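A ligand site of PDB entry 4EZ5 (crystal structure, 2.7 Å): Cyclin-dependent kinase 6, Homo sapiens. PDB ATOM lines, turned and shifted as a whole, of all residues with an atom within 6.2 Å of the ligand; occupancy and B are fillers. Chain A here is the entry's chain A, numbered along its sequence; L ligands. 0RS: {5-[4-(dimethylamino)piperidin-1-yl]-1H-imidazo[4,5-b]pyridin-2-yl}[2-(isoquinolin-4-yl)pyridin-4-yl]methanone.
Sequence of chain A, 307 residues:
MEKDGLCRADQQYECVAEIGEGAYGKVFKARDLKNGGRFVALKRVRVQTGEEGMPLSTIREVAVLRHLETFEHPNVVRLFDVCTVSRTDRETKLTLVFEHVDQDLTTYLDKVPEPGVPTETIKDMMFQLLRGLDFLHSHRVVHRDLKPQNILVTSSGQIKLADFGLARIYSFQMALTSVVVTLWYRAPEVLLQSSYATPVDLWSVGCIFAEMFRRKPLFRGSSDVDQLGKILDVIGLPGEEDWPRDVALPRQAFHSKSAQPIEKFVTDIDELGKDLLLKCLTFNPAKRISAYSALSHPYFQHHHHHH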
ATOM      1  N   GLU A  18     -16.251  14.345  34.917  1.00  0.00           N
ATOM      2  CA  GLU A  18     -16.800  15.569  34.364  1.00  0.00           C
ATOM      3  C   GLU A  18     -15.662  16.312  33.673  1.00  0.00           C
ATOM      4  O   GLU A  18     -14.532  16.317  34.162  1.00  0.00           O
ATOM      5  CB  GLU A  18     -17.411  16.444  35.468  1.00  0.00           C
ATOM      6  CG  GLU A  18     -18.130  17.680  34.929  1.00  0.00           C
ATOM      7  CD  GLU A  18     -18.561  18.640  36.034  1.00  0.00           C
ATOM      8  OE1 GLU A  18     -17.714  19.032  36.866  1.00  0.00           O
ATOM      9  OE2 GLU A  18     -19.762  19.012  36.057  1.00  0.00           O
ATOM     10  N   ILE A  19     -15.952  16.921  32.535  1.00  0.00           N
ATOM     11  CA  ILE A  19     -14.954  17.714  31.833  1.00  0.00           C
ATOM     12  C   ILE A  19     -15.013  19.158  32.326  1.00  0.00           C
ATOM     13  O   ILE A  19     -13.984  19.791  32.566  1.00  0.00           O
ATOM     14  CB  ILE A  19     -15.159  17.669  30.310  1.00  0.00           C
ATOM     15  CG1 ILE A  19     -15.160  16.222  29.819  1.00  0.00           C
ATOM     16  CG2 ILE A  19     -14.045  18.431  29.615  1.00  0.00           C
ATOM     17  CD1 ILE A  19     -15.214  16.092  28.312  1.00  0.00           C
ATOM     18  N   GLY A  25     -24.074  23.869  28.984  1.00  0.00           N
ATOM     19  CA  GLY A  25     -24.542  23.136  30.155  1.00  0.00           C
ATOM     20  C   GLY A  25     -23.459  22.320  30.820  1.00  0.00           C
ATOM     21  O   GLY A  25     -22.411  22.843  31.206  1.00  0.00           O
ATOM     22  N   VAL A  27     -20.936  18.838  30.754  1.00  0.00           N
ATOM     23  CA  VAL A  27     -20.282  17.853  29.893  1.00  0.00           C
ATOM     24  C   VAL A  27     -19.477  16.806  30.643  1.00  0.00           C
ATOM     25  O   VAL A  27     -18.696  17.126  31.533  1.00  0.00           O
ATOM     26  CB  VAL A  27     -19.347  18.533  28.862  1.00  0.00           C
ATOM     27  CG1 VAL A  27     -20.153  19.088  27.706  1.00  0.00           C
ATOM     28  CG2 VAL A  27     -18.543  19.639  29.525  1.00  0.00           C
ATOM     29  N   VAL A  40     -16.326   8.810  24.810  1.00  0.00           N
ATOM     30  CA  VAL A  40     -17.189   9.780  24.146  1.00  0.00           C
ATOM     31  C   VAL A  40     -17.422  10.980  25.057  1.00  0.00           C
ATOM     32  O   VAL A  40     -16.974  10.982  26.211  1.00  0.00           O
ATOM     33  CB  VAL A  40     -18.525   9.168  23.700  1.00  0.00           C
ATOM     34  CG1 VAL A  40     -18.306   8.212  22.553  1.00  0.00           C
ATOM     35  CG2 VAL A  40     -19.218   8.464  24.859  1.00  0.00           C
ATOM     36  N   ALA A  41     -18.091  12.008  24.541  1.00  0.00           N
ATOM     37  CA  ALA A  41     -18.447  13.171  25.332  1.00  0.00           C
ATOM     38  C   ALA A  41     -19.961  13.348  25.381  1.00  0.00           C
ATOM     39  O   ALA A  41     -20.597  13.470  24.339  1.00  0.00           O
ATOM     40  CB  ALA A  41     -17.767  14.406  24.784  1.00  0.00           C
ATOM     41  N   LYS A  43     -23.369  15.446  26.691  1.00  0.00           N
ATOM     42  CA  LYS A  43     -23.908  16.702  27.171  1.00  0.00           C
ATOM     43  C   LYS A  43     -25.406  16.533  27.282  1.00  0.00           C
ATOM     44  O   LYS A  43     -26.047  16.066  26.326  1.00  0.00           O
ATOM     45  CB  LYS A  43     -23.552  17.855  26.225  1.00  0.00           C
ATOM     46  CG  LYS A  43     -23.883  19.230  26.791  1.00  0.00           C
ATOM     47  CD  LYS A  43     -23.206  20.363  26.033  1.00  0.00           C
ATOM     48  CE  LYS A  43     -23.705  20.489  24.602  1.00  0.00           C
ATOM     49  NZ  LYS A  43     -23.331  21.803  23.962  1.00  0.00           N
ATOM     50  N   VAL A  77     -15.717  18.730  15.883  1.00  0.00           N
ATOM     51  CA  VAL A  77     -16.020  17.565  16.707  1.00  0.00           C
ATOM     52  C   VAL A  77     -17.149  16.719  16.093  1.00  0.00           C
ATOM     53  O   VAL A  77     -18.167  17.249  15.688  1.00  0.00           O
ATOM     54  CB  VAL A  77     -16.364  18.006  18.151  1.00  0.00           C
ATOM     55  CG1 VAL A  77     -17.528  17.224  18.701  1.00  0.00           C
ATOM     56  CG2 VAL A  77     -15.151  17.866  19.046  1.00  0.00           C
ATOM     57  N   ARG A  78     -16.922  15.408  16.016  1.00  0.00           N
ATOM     58  CA  ARG A  78     -17.920  14.482  15.455  1.00  0.00           C
ATOM     59  C   ARG A  78     -19.133  14.349  16.371  1.00  0.00           C
ATOM     60  O   ARG A  78     -18.986  14.254  17.588  1.00  0.00           O
ATOM     61  CB  ARG A  78     -17.323  13.078  15.239  1.00  0.00           C
ATOM     62  CG  ARG A  78     -16.193  12.948  14.197  1.00  0.00           C
ATOM     63  CD  ARG A  78     -16.691  12.955  12.753  1.00  0.00           C
ATOM     64  NE  ARG A  78     -17.178  14.282  12.364  1.00  0.00           N
ATOM     65  CZ  ARG A  78     -16.389  15.298  12.045  1.00  0.00           C
ATOM     66  NH1 ARG A  78     -16.908  16.474  11.721  1.00  0.00           N
ATOM     67  NH2 ARG A  78     -15.065  15.152  12.063  1.00  0.00           N
ATOM     68  N   PHE A  98     -20.940  13.200  21.571  1.00  0.00           N
ATOM     69  CA  PHE A  98     -19.901  13.620  20.636  1.00  0.00           C
ATOM     70  C   PHE A  98     -18.726  12.712  20.840  1.00  0.00           C
ATOM     71  O   PHE A  98     -18.731  11.864  21.723  1.00  0.00           O
ATOM     72  CB  PHE A  98     -19.483  15.059  20.931  1.00  0.00           C
ATOM     73  CG  PHE A  98     -20.565  16.074  20.755  1.00  0.00           C
ATOM     74  CD1 PHE A  98     -20.758  16.702  19.533  1.00  0.00           C
ATOM     75  CD2 PHE A  98     -21.387  16.406  21.811  1.00  0.00           C
ATOM     76  CE1 PHE A  98     -21.740  17.633  19.367  1.00  0.00           C
ATOM     77  CE2 PHE A  98     -22.383  17.350  21.658  1.00  0.00           C
ATOM     78  CZ  PHE A  98     -22.556  17.960  20.427  1.00  0.00           C
ATOM     79  N   GLU A  99     -17.684  12.904  20.044  1.00  0.00           N
ATOM     80  CA  GLU A  99     -16.458  12.190  20.275  1.00  0.00           C
ATOM     81  C   GLU A  99     -15.759  12.819  21.474  1.00  0.00           C
ATOM     82  O   GLU A  99     -16.204  13.831  21.995  1.00  0.00           O
ATOM     83  CB  GLU A  99     -15.561  12.228  19.045  1.00  0.00           C
ATOM     84  CG  GLU A  99     -15.235  13.618  18.597  1.00  0.00           C
ATOM     85  CD  GLU A  99     -14.268  13.628  17.447  1.00  0.00           C
ATOM     86  OE1 GLU A  99     -14.244  14.626  16.697  1.00  0.00           O
ATOM     87  OE2 GLU A  99     -13.531  12.646  17.310  1.00  0.00           O
ATOM     88  N   HIS A 100     -14.682  12.191  21.934  1.00  0.00           N
ATOM     89  CA  HIS A 100     -13.900  12.744  23.022  1.00  0.00           C
ATOM     90  C   HIS A 100     -12.521  13.050  22.484  1.00  0.00           C
ATOM     91  O   HIS A 100     -11.999  12.306  21.659  1.00  0.00           O
ATOM     92  CB  HIS A 100     -13.861  11.761  24.205  1.00  0.00           C
ATOM     93  CG  HIS A 100     -13.030  12.212  25.357  1.00  0.00           C
ATOM     94  ND1 HIS A 100     -11.655  12.191  25.338  1.00  0.00           N
ATOM     95  CD2 HIS A 100     -13.379  12.696  26.572  1.00  0.00           C
ATOM     96  CE1 HIS A 100     -11.180  12.639  26.488  1.00  0.00           C
ATOM     97  NE2 HIS A 100     -12.212  12.956  27.251  1.00  0.00           N
ATOM     98  N   VAL A 101     -11.938  14.155  22.912  1.00  0.00           N
ATOM     99  CA  VAL A 101     -10.568  14.519  22.551  1.00  0.00           C
ATOM    100  C   VAL A 101      -9.754  14.655  23.832  1.00  0.00           C
ATOM    101  O   VAL A 101     -10.267  15.144  24.841  1.00  0.00           O
ATOM    102  CB  VAL A 101     -10.521  15.832  21.751  1.00  0.00           C
ATOM    103  CG1 VAL A 101      -9.108  16.199  21.394  1.00  0.00           C
ATOM    104  CG2 VAL A 101     -11.368  15.726  20.515  1.00  0.00           C
ATOM    105  N   ASP A 102      -8.506  14.206  23.820  1.00  0.00           N
ATOM    106  CA  ASP A 102      -7.721  14.117  25.070  1.00  0.00           C
ATOM    107  C   ASP A 102      -7.506  15.466  25.773  1.00  0.00           C
ATOM    108  O   ASP A 102      -7.371  15.510  27.003  1.00  0.00           O
ATOM    109  CB  ASP A 102      -6.372  13.427  24.822  1.00  0.00           C
ATOM    110  CG  ASP A 102      -6.516  11.939  24.485  1.00  0.00           C
ATOM    111  OD1 ASP A 102      -7.324  11.615  23.586  1.00  0.00           O
ATOM    112  OD2 ASP A 102      -5.823  11.108  25.117  1.00  0.00           O
ATOM    113  N   GLN A 103      -7.485  16.556  25.010  1.00  0.00           N
ATOM    114  CA  GLN A 103      -7.172  17.854  25.587  1.00  0.00           C
ATOM    115  C   GLN A 103      -7.638  19.044  24.750  1.00  0.00           C
ATOM    116  O   GLN A 103      -7.952  18.903  23.569  1.00  0.00           O
ATOM    117  CB  GLN A 103      -5.663  17.960  25.827  1.00  0.00           C
ATOM    118  CG  GLN A 103      -4.862  18.205  24.579  1.00  0.00           C
ATOM    119  CD  GLN A 103      -3.380  18.270  24.858  1.00  0.00           C
ATOM    120  OE1 GLN A 103      -2.922  17.814  25.900  1.00  0.00           O
ATOM    121  NE2 GLN A 103      -2.628  18.862  23.939  1.00  0.00           N
ATOM    122  N   ASP A 104      -7.686  20.215  25.378  1.00  0.00           N
ATOM    123  CA  ASP A 104      -8.072  21.439  24.681  1.00  0.00           C
ATOM    124  C   ASP A 104      -6.843  22.229  24.286  1.00  0.00           C
ATOM    125  O   ASP A 104      -5.727  21.775  24.519  1.00  0.00           O
ATOM    126  CB  ASP A 104      -9.031  22.300  25.533  1.00  0.00           C
ATOM    127  CG  ASP A 104      -8.399  22.820  26.814  1.00  0.00           C
ATOM    128  OD1 ASP A 104      -7.188  23.105  26.828  1.00  0.00           O
ATOM    129  OD2 ASP A 104      -9.129  22.955  27.817  1.00  0.00           O
ATOM    130  N   THR A 107      -4.713  23.438  27.666  1.00  0.00           N
ATOM    131  CA  THR A 107      -3.761  22.548  28.311  1.00  0.00           C
ATOM    132  C   THR A 107      -2.565  22.280  27.397  1.00  0.00           C
ATOM    133  O   THR A 107      -1.457  22.055  27.859  1.00  0.00           O
ATOM    134  CB  THR A 107      -4.388  21.215  28.811  1.00  0.00           C
ATOM    135  OG1 THR A 107      -4.053  20.152  27.910  1.00  0.00           O
ATOM    136  CG2 THR A 107      -5.894  21.338  28.938  1.00  0.00           C
ATOM    137  N   LYS A 147     -13.018  30.346  22.139  1.00  0.00           N
ATOM    138  CA  LYS A 147     -11.947  30.560  23.091  1.00  0.00           C
ATOM    139  C   LYS A 147     -11.146  29.262  23.112  1.00  0.00           C
ATOM    140  O   LYS A 147     -11.664  28.222  22.706  1.00  0.00           O
ATOM    141  CB  LYS A 147     -12.528  30.869  24.477  1.00  0.00           C
ATOM    142  CG  LYS A 147     -13.365  29.739  25.043  1.00  0.00           C
ATOM    143  CD  LYS A 147     -14.279  30.178  26.174  1.00  0.00           C
ATOM    144  CE  LYS A 147     -15.497  29.253  26.229  1.00  0.00           C
ATOM    145  NZ  LYS A 147     -16.370  29.455  27.426  1.00  0.00           N
ATOM    146  N   GLN A 149     -10.549  27.270  25.300  1.00  0.00           N
ATOM    147  CA  GLN A 149     -11.147  26.289  26.189  1.00  0.00           C
ATOM    148  C   GLN A 149     -12.150  25.370  25.467  1.00  0.00           C
ATOM    149  O   GLN A 149     -12.598  24.373  26.034  1.00  0.00           O
ATOM    150  CB  GLN A 149     -11.815  26.970  27.388  1.00  0.00           C
ATOM    151  CG  GLN A 149     -10.853  27.691  28.356  1.00  0.00           C
ATOM    152  CD  GLN A 149     -10.394  29.059  27.851  1.00  0.00           C
ATOM    153  OE1 GLN A 149     -10.766  29.492  26.758  1.00  0.00           O
ATOM    154  NE2 GLN A 149      -9.590  29.758  28.659  1.00  0.00           N
ATOM    155  N   ASN A 150     -12.510  25.706  24.234  1.00  0.00           N
ATOM    156  CA  ASN A 150     -13.337  24.804  23.412  1.00  0.00           C
ATOM    157  C   ASN A 150     -12.723  24.521  22.052  1.00  0.00           C
ATOM    158  O   ASN A 150     -13.386  24.049  21.124  1.00  0.00           O
ATOM    159  CB  ASN A 150     -14.794  25.288  23.305  1.00  0.00           C
ATOM    160  CG  ASN A 150     -14.907  26.765  22.983  1.00  0.00           C
ATOM    161  OD1 ASN A 150     -14.115  27.322  22.226  1.00  0.00           O
ATOM    162  ND2 ASN A 150     -15.921  27.406  23.559  1.00  0.00           N
ATOM    163  N   ILE A 151     -11.437  24.827  21.929  1.00  0.00           N
ATOM    164  CA  ILE A 151     -10.680  24.387  20.776  1.00  0.00           C
ATOM    165  C   ILE A 151      -9.906  23.134  21.162  1.00  0.00           C
ATOM    166  O   ILE A 151      -8.948  23.184  21.932  1.00  0.00           O
ATOM    167  CB  ILE A 151      -9.704  25.462  20.346  1.00  0.00           C
ATOM    168  CG1 ILE A 151     -10.477  26.681  19.849  1.00  0.00           C
ATOM    169  CG2 ILE A 151      -8.793  24.912  19.265  1.00  0.00           C
ATOM    170  CD1 ILE A 151      -9.598  27.841  19.500  1.00  0.00           C
ATOM    171  N   LEU A 152     -10.336  21.989  20.646  1.00  0.00           N
ATOM    172  CA  LEU A 152      -9.784  20.714  21.063  1.00  0.00           C
ATOM    173  C   LEU A 152      -8.643  20.233  20.173  1.00  0.00           C
ATOM    174  O   LEU A 152      -8.723  20.338  18.953  1.00  0.00           O
ATOM    175  CB  LEU A 152     -10.898  19.662  21.089  1.00  0.00           C
ATOM    176  CG  LEU A 152     -12.126  20.093  21.898  1.00  0.00           C
ATOM    177  CD1 LEU A 152     -13.112  18.964  21.963  1.00  0.00           C
ATOM    178  CD2 LEU A 152     -11.707  20.537  23.288  1.00  0.00           C
ATOM    179  N   ALA A 162     -15.293  22.711  19.223  1.00  0.00           N
ATOM    180  CA  ALA A 162     -16.392  22.218  20.051  1.00  0.00           C
ATOM    181  C   ALA A 162     -17.274  23.369  20.536  1.00  0.00           C
ATOM    182  O   ALA A 162     -16.930  24.528  20.355  1.00  0.00           O
ATOM    183  CB  ALA A 162     -15.856  21.421  21.220  1.00  0.00           C
ATOM    184  N   ASP A 163     -18.409  23.022  21.153  1.00  0.00           N
ATOM    185  CA  ASP A 163     -19.247  23.981  21.868  1.00  0.00           C
ATOM    186  C   ASP A 163     -19.867  25.076  20.999  1.00  0.00           C
ATOM    187  O   ASP A 163     -19.674  26.270  21.234  1.00  0.00           O
ATOM    188  CB  ASP A 163     -18.460  24.625  23.014  1.00  0.00           C
ATOM    189  CG  ASP A 163     -19.328  25.491  23.908  1.00  0.00           C
ATOM    190  OD1 ASP A 163     -20.525  25.167  24.069  1.00  0.00           O
ATOM    191  OD2 ASP A 163     -18.809  26.498  24.426  1.00  0.00           O
ATOM    192  N   PHE A 164     -20.639  24.676  19.995  1.00  0.00           N
ATOM    193  CA  PHE A 164     -21.258  25.652  19.112  1.00  0.00           C
ATOM    194  C   PHE A 164     -22.671  25.249  18.710  1.00  0.00           C
ATOM    195  O   PHE A 164     -23.055  24.083  18.879  1.00  0.00           O
ATOM    196  CB  PHE A 164     -20.377  25.910  17.889  1.00  0.00           C
ATOM    197  CG  PHE A 164     -20.093  24.674  17.076  1.00  0.00           C
ATOM    198  CD1 PHE A 164     -20.952  24.281  16.061  1.00  0.00           C
ATOM    199  CD2 PHE A 164     -18.961  23.910  17.326  1.00  0.00           C
ATOM    200  CE1 PHE A 164     -20.696  23.138  15.318  1.00  0.00           C
ATOM    201  CE2 PHE A 164     -18.691  22.769  16.586  1.00  0.00           C
ATOM    202  CZ  PHE A 164     -19.561  22.384  15.576  1.00  0.00           C
HETATM  203  C1  0RS L   1      -7.620  18.358  34.183  1.00  0.00           C
HETATM  204  C2  0RS L   1      -9.994  18.365  33.853  1.00  0.00           C
HETATM  205  C3  0RS L   1      -8.460  18.232  31.903  1.00  0.00           C
HETATM  206  O1  0RS L   1     -14.205  15.653  24.125  1.00  0.00           O
HETATM  207  C11 0RS L   1     -12.572  19.059  26.577  1.00  0.00           C
HETATM  208  C12 0RS L   1     -13.528  17.552  25.388  1.00  0.00           C
HETATM  209  C13 0RS L   1     -11.890  17.849  26.848  1.00  0.00           C
HETATM  210  C14 0RS L   1     -14.436  16.812  24.423  1.00  0.00           C
HETATM  211  C15 0RS L   1     -15.626  17.499  23.834  1.00  0.00           C
HETATM  212  C16 0RS L   1     -16.188  17.030  22.638  1.00  0.00           C
HETATM  213  C17 0RS L   1     -17.308  17.703  22.123  1.00  0.00           C
HETATM  214  C18 0RS L   1     -17.354  19.241  23.853  1.00  0.00           C
HETATM  215  C19 0RS L   1     -16.249  18.612  24.447  1.00  0.00           C
HETATM  216  C20 0RS L   1     -18.029  20.411  24.460  1.00  0.00           C
HETATM  217  C21 0RS L   1     -19.443  20.435  24.431  1.00  0.00           C
HETATM  218  C22 0RS L   1     -19.576  22.435  25.528  1.00  0.00           C
HETATM  219  C23 0RS L   1     -18.179  22.546  25.637  1.00  0.00           C
HETATM  220  C24 0RS L   1     -17.587  23.655  26.257  1.00  0.00           C
HETATM  221  C25 0RS L   1     -16.175  23.741  26.358  1.00  0.00           C
HETATM  222  C26 0RS L   1     -15.356  22.731  25.833  1.00  0.00           C
HETATM  223  C27 0RS L   1     -15.959  21.630  25.196  1.00  0.00           C
HETATM  224  C28 0RS L   1     -17.380  21.512  25.092  1.00  0.00           C
HETATM  225  N1  0RS L   1      -8.709  17.904  33.320  1.00  0.00           N
HETATM  226  C4  0RS L   1      -8.924  17.088  30.972  1.00  0.00           C
HETATM  227  C5  0RS L   1      -8.675  17.437  29.491  1.00  0.00           C
HETATM  228  N2  0RS L   1      -9.376  18.686  29.187  1.00  0.00           N
HETATM  229  C6  0RS L   1      -8.820  19.795  29.952  1.00  0.00           C
HETATM  230  C7  0RS L   1      -9.033  19.587  31.462  1.00  0.00           C
HETATM  231  C8  0RS L   1     -10.429  18.788  28.330  1.00  0.00           C
HETATM  232  C9  0RS L   1     -11.034  20.056  28.143  1.00  0.00           C
HETATM  233  C10 0RS L   1     -12.113  20.204  27.249  1.00  0.00           C
HETATM  234  N3  0RS L   1     -13.590  18.867  25.658  1.00  0.00           N
HETATM  235  N4  0RS L   1     -12.544  16.911  26.067  1.00  0.00           N
HETATM  236  N5  0RS L   1     -10.844  17.662  27.700  1.00  0.00           N
HETATM  237  N6  0RS L   1     -17.874  18.780  22.713  1.00  0.00           N
HETATM  238  N7  0RS L   1     -20.207  21.412  24.942  1.00  0.00           N
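An oxygen (O1) of the ligand lies close to the backbone carbonyl oxygen (O) of Glu 99, 3.4 Å away.
Residues that only touch the ligand: Ile 19, Val 27, Ala 41, Val 77, Phe 98, His 100, Asp 102, Asp 104, Thr 107, Gln 149, Asn 150, Leu 152, Ala 162 and Asp 163.
Hydrophobic or aromatic side chains within 4 Å of the ligand: Ile 19, Val 27, Ala 41, Val 77, Phe 98, His 100, Leu 152 and Ala 162.
OD2 of Asp 163 sits at hydrogen-bond distance from ND2 of Asn 150 (3.1 Å).
OE1 of Glu 99 is in hydrogen-bond range of N of Arg 78 (2.9 Å).
O of Val 27 is in hydrogen-bond range of N of Ile 19.
N of Thr 107 lies within hydrogen-bond range of OD1 of Asp 104 (2.6 Å).
The side-chain hydroxyl (OG1) of Thr 107 sits at hydrogen-bond distance from the side-chain amide oxygen (OE1) of Gln 103 (3.3 Å).
The backbone NH (N) of Phe 98 is in hydrogen-bond range of the backbone carbonyl oxygen (O) of Ala 41.
The backbone carbonyl oxygen (O) of Asn 150 sits at hydrogen-bond distance from the backbone NH (N) of Ala 162, 3.0 Å away.
The side-chain amide oxygen (OD1) of Asn 150 sits close to the backbone carbonyl oxygen (O) of Lys 147, 2.7 Å away.
An oxygen (O1) of the ligand lies within hydrogen-bond range of the backbone NH (N) of Val 101 (3.0 Å).
O of Val 101 sits close to N4 of the ligand (3.1 Å).
The side-chain amino group of Lys 43 is in hydrogen-bond range of a nitrogen (N7) of the ligand (3.3 Å).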
